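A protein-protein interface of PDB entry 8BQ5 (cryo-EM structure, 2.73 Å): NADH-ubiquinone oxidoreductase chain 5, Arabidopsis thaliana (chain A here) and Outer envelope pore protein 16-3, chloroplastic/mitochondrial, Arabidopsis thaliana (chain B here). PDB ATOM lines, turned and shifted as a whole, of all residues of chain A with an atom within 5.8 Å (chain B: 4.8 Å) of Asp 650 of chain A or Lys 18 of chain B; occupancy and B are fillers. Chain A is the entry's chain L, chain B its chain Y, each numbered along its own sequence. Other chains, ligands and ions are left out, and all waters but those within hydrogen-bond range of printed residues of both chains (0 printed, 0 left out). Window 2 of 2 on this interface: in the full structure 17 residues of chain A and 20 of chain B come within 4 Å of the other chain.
The side-chain carboxylate of Asp 650 of chain A is in salt-bridge range of the side-chain amino group of Lys 18 of chain B (3.6 Å).
The backbone carbonyl oxygen of Trp 648 of chain A lies close to the backbone carbonyl oxygen of Lys 21 of chain B (3.4 Å).
Hydrophobic or aromatic side chains of chain A within 4 Å of the printed part of chain B: Trp 648 and Leu 653.
Of the 12 printed residues of chain B, 4 touch a printed residue of chain A.
Hydrophobic or aromatic side chains of chain B that line the printed part of chain A: Ile 77.
Among the printed residues, 4 pairs touch across the chains.
Among the printed residues, Asp or Glu carboxylates within 4 Å of a Lys or Arg side-chain nitrogen of the other chain: Asp 650 of chain A with Lys 18 of chain B.
The backbone carbonyl oxygen (O) of Ile 77 of chain B sits close to the side-chain amide oxygen (OE1) of Gln 81 of chain B, at 3.0 Å.
Among the printed residues, pairs that only touch across the chains: Leu 653 of chain A with Gly 22 of chain B and Leu 653 of chain A with Ile 77 of chain B.
Of the printed residues of chain B, Asp 650 of chain A touches Lys 18 (3.6 Å).
Lys 18 of chain B touches one residue of chain A.
Printed residues of chain B within 4 Å of Leu 653 of chain A: Gly 22 and Ile 77.
Printed residues of chain A within 4 Å of Lys 21 of chain B: Trp 648 (3.4 Å).
Printed residues of chain A within 4 Å of Gly 22 of chain B: Leu 653 (3.7 Å).
Printed residues of chain A within 4 Å of Ile 77 of chain B: Leu 653.
Printed residues of chain B within 4 Å of Trp 648 of chain A: Lys 21 (3.4 Å).
Val 649 of chain A touches none of the printed residues of chain B.
Gly 14 of chain B touches none of the printed residues of chain A.
The nearest residue of chain B that does not touch Asp 650 of chain A is Ile 77 of chain B (4.5 Å).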
ATOM      1  N   LEU A 645       6.373 -14.234   8.799  1.00  0.00           N
ATOM      2  CA  LEU A 645       5.967 -14.500   7.424  1.00  0.00           C
ATOM      3  C   LEU A 645       7.111 -14.267   6.446  1.00  0.00           C
ATOM      4  O   LEU A 645       7.119 -14.852   5.358  1.00  0.00           O
ATOM      5  CB  LEU A 645       4.765 -13.638   7.045  1.00  0.00           C
ATOM      6  CG  LEU A 645       3.401 -14.119   7.542  1.00  0.00           C
ATOM      7  CD1 LEU A 645       2.281 -13.490   6.729  1.00  0.00           C
ATOM      8  CD2 LEU A 645       3.315 -15.636   7.501  1.00  0.00           C
ATOM      9  N   SER A 646       8.082 -13.429   6.815  1.00  0.00           N
ATOM     10  CA  SER A 646       9.171 -13.096   5.904  1.00  0.00           C
ATOM     11  C   SER A 646      10.031 -14.303   5.553  1.00  0.00           C
ATOM     12  O   SER A 646      10.743 -14.270   4.544  1.00  0.00           O
ATOM     13  CB  SER A 646      10.035 -11.990   6.509  1.00  0.00           C
ATOM     14  OG  SER A 646       9.229 -10.931   6.994  1.00  0.00           O
ATOM     15  N   TRP A 648       8.877 -17.074   4.530  1.00  0.00           N
ATOM     16  CA  TRP A 648       8.221 -17.712   3.395  1.00  0.00           C
ATOM     17  C   TRP A 648       7.888 -16.751   2.265  1.00  0.00           C
ATOM     18  O   TRP A 648       7.608 -17.200   1.149  1.00  0.00           O
ATOM     19  CB  TRP A 648       6.926 -18.400   3.844  1.00  0.00           C
ATOM     20  CG  TRP A 648       7.085 -19.844   4.199  1.00  0.00           C
ATOM     21  CD1 TRP A 648       6.776 -20.919   3.418  1.00  0.00           C
ATOM     22  CD2 TRP A 648       7.574 -20.375   5.435  1.00  0.00           C
ATOM     23  NE1 TRP A 648       7.049 -22.085   4.088  1.00  0.00           N
ATOM     24  CE2 TRP A 648       7.540 -21.779   5.329  1.00  0.00           C
ATOM     25  CE3 TRP A 648       8.042 -19.799   6.619  1.00  0.00           C
ATOM     26  CZ2 TRP A 648       7.955 -22.615   6.361  1.00  0.00           C
ATOM     27  CZ3 TRP A 648       8.453 -20.631   7.643  1.00  0.00           C
ATOM     28  CH2 TRP A 648       8.407 -22.023   7.508  1.00  0.00           C
ATOM     29  N   VAL A 649       7.909 -15.447   2.518  1.00  0.00           N
ATOM     30  CA  VAL A 649       7.428 -14.466   1.560  1.00  0.00           C
ATOM     31  C   VAL A 649       8.573 -13.549   1.144  1.00  0.00           C
ATOM     32  O   VAL A 649       9.655 -13.550   1.730  1.00  0.00           O
ATOM     33  CB  VAL A 649       6.252 -13.644   2.118  1.00  0.00           C
ATOM     34  CG1 VAL A 649       5.225 -14.556   2.766  1.00  0.00           C
ATOM     35  CG2 VAL A 649       6.762 -12.601   3.102  1.00  0.00           C
ATOM     36  N   ASP A 650       8.314 -12.756   0.109  1.00  0.00           N
ATOM     37  CA  ASP A 650       9.204 -11.692  -0.321  1.00  0.00           C
ATOM     38  C   ASP A 650       8.359 -10.466  -0.628  1.00  0.00           C
ATOM     39  O   ASP A 650       7.265 -10.578  -1.187  1.00  0.00           O
ATOM     40  CB  ASP A 650      10.019 -12.099  -1.554  1.00  0.00           C
ATOM     41  CG  ASP A 650      11.072 -13.137  -1.234  1.00  0.00           C
ATOM     42  OD1 ASP A 650      11.368 -13.334  -0.036  1.00  0.00           O
ATOM     43  OD2 ASP A 650      11.613 -13.748  -2.178  1.00  0.00           O
ATOM     44  N   ASN A 651       8.870  -9.290  -0.251  1.00  0.00           N
ATOM     45  CA  ASN A 651       8.156  -8.055  -0.562  1.00  0.00           C
ATOM     46  C   ASN A 651       7.962  -7.893  -2.062  1.00  0.00           C
ATOM     47  O   ASN A 651       7.019  -7.224  -2.499  1.00  0.00           O
ATOM     48  CB  ASN A 651       8.905  -6.851   0.003  1.00  0.00           C
ATOM     49  CG  ASN A 651       8.801  -6.755   1.509  1.00  0.00           C
ATOM     50  OD1 ASN A 651       8.153  -7.581   2.153  1.00  0.00           O
ATOM     51  ND2 ASN A 651       9.437  -5.741   2.081  1.00  0.00           N
ATOM     52  N   ARG A 652       8.847  -8.496  -2.855  1.00  0.00           N
ATOM     53  CA  ARG A 652       8.690  -8.505  -4.304  1.00  0.00           C
ATOM     54  C   ARG A 652       7.418  -9.240  -4.709  1.00  0.00           C
ATOM     55  O   ARG A 652       6.588  -8.712  -5.456  1.00  0.00           O
ATOM     56  CB  ARG A 652       9.913  -9.165  -4.934  1.00  0.00           C
ATOM     57  CG  ARG A 652      11.117  -9.171  -4.011  1.00  0.00           C
ATOM     58  CD  ARG A 652      12.377  -9.552  -4.743  1.00  0.00           C
ATOM     59  NE  ARG A 652      12.517  -8.823  -5.996  1.00  0.00           N
ATOM     60  CZ  ARG A 652      13.457  -9.070  -6.897  1.00  0.00           C
ATOM     61  NH1 ARG A 652      14.362 -10.015  -6.707  1.00  0.00           N
ATOM     62  NH2 ARG A 652      13.493  -8.346  -8.011  1.00  0.00           N
ATOM     63  N   LEU A 653       7.244 -10.463  -4.203  1.00  0.00           N
ATOM     64  CA  LEU A 653       6.119 -11.293  -4.621  1.00  0.00           C
ATOM     65  C   LEU A 653       4.800 -10.730  -4.114  1.00  0.00           C
ATOM     66  O   LEU A 653       3.744 -10.953  -4.717  1.00  0.00           O
ATOM     67  CB  LEU A 653       6.300 -12.730  -4.127  1.00  0.00           C
ATOM     68  CG  LEU A 653       7.485 -13.503  -4.714  1.00  0.00           C
ATOM     69  CD1 LEU A 653       7.634 -14.854  -4.031  1.00  0.00           C
ATOM     70  CD2 LEU A 653       7.327 -13.671  -6.217  1.00  0.00           C
ATOM     71  N   SER A 654       4.836 -10.005  -2.994  1.00  0.00           N
ATOM     72  CA  SER A 654       3.619  -9.407  -2.469  1.00  0.00           C
ATOM     73  C   SER A 654       3.004  -8.461  -3.491  1.00  0.00           C
ATOM     74  O   SER A 654       1.863  -8.653  -3.919  1.00  0.00           O
ATOM     75  CB  SER A 654       3.913  -8.681  -1.151  1.00  0.00           C
ATOM     76  OG  SER A 654       3.685  -9.532  -0.039  1.00  0.00           O
ATOM     77  N   PHE A 655       3.785  -7.483  -3.959  1.00  0.00           N
ATOM     78  CA  PHE A 655       3.244  -6.480  -4.872  1.00  0.00           C
ATOM     79  C   PHE A 655       3.076  -7.043  -6.277  1.00  0.00           C
ATOM     80  O   PHE A 655       2.286  -6.519  -7.070  1.00  0.00           O
ATOM     81  CB  PHE A 655       4.136  -5.239  -4.882  1.00  0.00           C
ATOM     82  CG  PHE A 655       3.986  -4.376  -3.658  1.00  0.00           C
ATOM     83  CD1 PHE A 655       3.646  -3.042  -3.772  1.00  0.00           C
ATOM     84  CD2 PHE A 655       4.195  -4.900  -2.393  1.00  0.00           C
ATOM     85  CE1 PHE A 655       3.511  -2.247  -2.651  1.00  0.00           C
ATOM     86  CE2 PHE A 655       4.062  -4.111  -1.268  1.00  0.00           C
ATOM     87  CZ  PHE A 655       3.718  -2.783  -1.395  1.00  0.00           C
ATOM     88  N   ASP B  13      18.514 -18.017   2.004  1.00  0.00           N
ATOM     89  CA  ASP B  13      18.414 -18.184   0.557  1.00  0.00           C
ATOM     90  C   ASP B  13      18.226 -19.637   0.137  1.00  0.00           C
ATOM     91  O   ASP B  13      17.723 -20.460   0.909  1.00  0.00           O
ATOM     92  CB  ASP B  13      19.653 -17.599  -0.126  1.00  0.00           C
ATOM     93  CG  ASP B  13      19.563 -16.098  -0.310  1.00  0.00           C
ATOM     94  OD1 ASP B  13      18.503 -15.522   0.007  1.00  0.00           O
ATOM     95  OD2 ASP B  13      20.555 -15.493  -0.768  1.00  0.00           O
ATOM     96  N   GLY B  14      18.637 -19.955  -1.089  1.00  0.00           N
ATOM     97  CA  GLY B  14      18.423 -21.259  -1.671  1.00  0.00           C
ATOM     98  C   GLY B  14      17.438 -21.181  -2.820  1.00  0.00           C
ATOM     99  O   GLY B  14      16.221 -21.126  -2.617  1.00  0.00           O
ATOM    100  N   PRO B  15      17.954 -21.173  -4.055  1.00  0.00           N
ATOM    101  CA  PRO B  15      17.079 -20.912  -5.216  1.00  0.00           C
ATOM    102  C   PRO B  15      15.912 -21.877  -5.333  1.00  0.00           C
ATOM    103  O   PRO B  15      14.784 -21.452  -5.622  1.00  0.00           O
ATOM    104  CB  PRO B  15      18.035 -21.037  -6.413  1.00  0.00           C
ATOM    105  CG  PRO B  15      19.410 -20.917  -5.846  1.00  0.00           C
ATOM    106  CD  PRO B  15      19.354 -21.413  -4.441  1.00  0.00           C
ATOM    107  N   LEU B  16      16.151 -23.169  -5.104  1.00  0.00           N
ATOM    108  CA  LEU B  16      15.055 -24.131  -5.095  1.00  0.00           C
ATOM    109  C   LEU B  16      14.098 -23.855  -3.943  1.00  0.00           C
ATOM    110  O   LEU B  16      12.872 -23.890  -4.117  1.00  0.00           O
ATOM    111  CB  LEU B  16      15.620 -25.547  -5.012  1.00  0.00           C
ATOM    112  CG  LEU B  16      14.777 -26.650  -4.377  1.00  0.00           C
ATOM    113  CD1 LEU B  16      13.603 -27.032  -5.267  1.00  0.00           C
ATOM    114  CD2 LEU B  16      15.661 -27.851  -4.098  1.00  0.00           C
ATOM    115  N   MET B  17      14.641 -23.570  -2.758  1.00  0.00           N
ATOM    116  CA  MET B  17      13.788 -23.217  -1.630  1.00  0.00           C
ATOM    117  C   MET B  17      13.060 -21.907  -1.889  1.00  0.00           C
ATOM    118  O   MET B  17      11.896 -21.750  -1.502  1.00  0.00           O
ATOM    119  CB  MET B  17      14.609 -23.136  -0.343  1.00  0.00           C
ATOM    120  CG  MET B  17      13.752 -23.106   0.910  1.00  0.00           C
ATOM    121  SD  MET B  17      13.318 -24.756   1.489  1.00  0.00           S
ATOM    122  CE  MET B  17      11.697 -24.456   2.188  1.00  0.00           C
ATOM    123  N   LYS B  18      13.729 -20.955  -2.545  1.00  0.00           N
ATOM    124  CA  LYS B  18      13.067 -19.709  -2.919  1.00  0.00           C
ATOM    125  C   LYS B  18      11.864 -19.973  -3.814  1.00  0.00           C
ATOM    126  O   LYS B  18      10.777 -19.435  -3.581  1.00  0.00           O
ATOM    127  CB  LYS B  18      14.056 -18.770  -3.613  1.00  0.00           C
ATOM    128  CG  LYS B  18      15.031 -18.080  -2.678  1.00  0.00           C
ATOM    129  CD  LYS B  18      14.289 -17.195  -1.693  1.00  0.00           C
ATOM    130  CE  LYS B  18      15.081 -15.943  -1.355  1.00  0.00           C
ATOM    131  NZ  LYS B  18      14.439 -15.172  -0.253  1.00  0.00           N
ATOM    132  N   THR B  19      12.036 -20.811  -4.841  1.00  0.00           N
ATOM    133  CA  THR B  19      10.923 -21.103  -5.740  1.00  0.00           C
ATOM    134  C   THR B  19       9.797 -21.834  -5.016  1.00  0.00           C
ATOM    135  O   THR B  19       8.617 -21.512  -5.209  1.00  0.00           O
ATOM    136  CB  THR B  19      11.408 -21.919  -6.940  1.00  0.00           C
ATOM    137  OG1 THR B  19      11.989 -21.038  -7.906  1.00  0.00           O
ATOM    138  CG2 THR B  19      10.248 -22.667  -7.588  1.00  0.00           C
ATOM    139  N   ILE B  20      10.138 -22.814  -4.175  1.00  0.00           N
ATOM    140  CA  ILE B  20       9.106 -23.574  -3.471  1.00  0.00           C
ATOM    141  C   ILE B  20       8.311 -22.659  -2.547  1.00  0.00           C
ATOM    142  O   ILE B  20       7.072 -22.668  -2.544  1.00  0.00           O
ATOM    143  CB  ILE B  20       9.735 -24.748  -2.698  1.00  0.00           C
ATOM    144  CG1 ILE B  20      10.351 -25.773  -3.657  1.00  0.00           C
ATOM    145  CG2 ILE B  20       8.700 -25.418  -1.811  1.00  0.00           C
ATOM    146  CD1 ILE B  20       9.593 -25.961  -4.957  1.00  0.00           C
ATOM    147  N   LYS B  21       9.012 -21.841  -1.758  1.00  0.00           N
ATOM    148  CA  LYS B  21       8.330 -20.949  -0.830  1.00  0.00           C
ATOM    149  C   LYS B  21       7.531 -19.879  -1.561  1.00  0.00           C
ATOM    150  O   LYS B  21       6.451 -19.496  -1.098  1.00  0.00           O
ATOM    151  CB  LYS B  21       9.338 -20.310   0.122  1.00  0.00           C
ATOM    152  CG  LYS B  21       9.796 -21.228   1.243  1.00  0.00           C
ATOM    153  CD  LYS B  21      10.847 -20.551   2.104  1.00  0.00           C
ATOM    154  CE  LYS B  21      10.883 -21.144   3.502  1.00  0.00           C
ATOM    155  NZ  LYS B  21      11.867 -20.439   4.370  1.00  0.00           N
ATOM    156  N   GLY B  22       8.039 -19.380  -2.691  1.00  0.00           N
ATOM    157  CA  GLY B  22       7.260 -18.449  -3.488  1.00  0.00           C
ATOM    158  C   GLY B  22       5.976 -19.062  -4.005  1.00  0.00           C
ATOM    159  O   GLY B  22       4.918 -18.430  -3.969  1.00  0.00           O
ATOM    160  N   ILE B  77       9.806 -16.149  -9.316  1.00  0.00           N
ATOM    161  CA  ILE B  77      11.035 -16.345  -8.555  1.00  0.00           C
ATOM    162  C   ILE B  77      11.983 -17.297  -9.272  1.00  0.00           C
ATOM    163  O   ILE B  77      13.201 -17.064  -9.305  1.00  0.00           O
ATOM    164  CB  ILE B  77      10.698 -16.841  -7.136  1.00  0.00           C
ATOM    165  CG1 ILE B  77       9.845 -15.804  -6.407  1.00  0.00           C
ATOM    166  CG2 ILE B  77      11.964 -17.119  -6.344  1.00  0.00           C
ATOM    167  CD1 ILE B  77      10.441 -14.415  -6.426  1.00  0.00           C
ATOM    168  N   GLN B  81      15.747 -16.253 -10.537  1.00  0.00           N
ATOM    169  CA  GLN B  81      16.979 -16.888 -10.079  1.00  0.00           C
ATOM    170  C   GLN B  81      17.751 -17.505 -11.237  1.00  0.00           C
ATOM    171  O   GLN B  81      18.979 -17.377 -11.308  1.00  0.00           O
ATOM    172  CB  GLN B  81      16.670 -17.942  -9.019  1.00  0.00           C
ATOM    173  CG  GLN B  81      17.152 -17.566  -7.630  1.00  0.00           C
ATOM    174  CD  GLN B  81      16.285 -16.507  -6.980  1.00  0.00           C
ATOM    175  OE1 GLN B  81      15.058 -16.581  -7.026  1.00  0.00           O
ATOM    176  NE2 GLN B  81      16.920 -15.514  -6.366  1.00  0.00           N
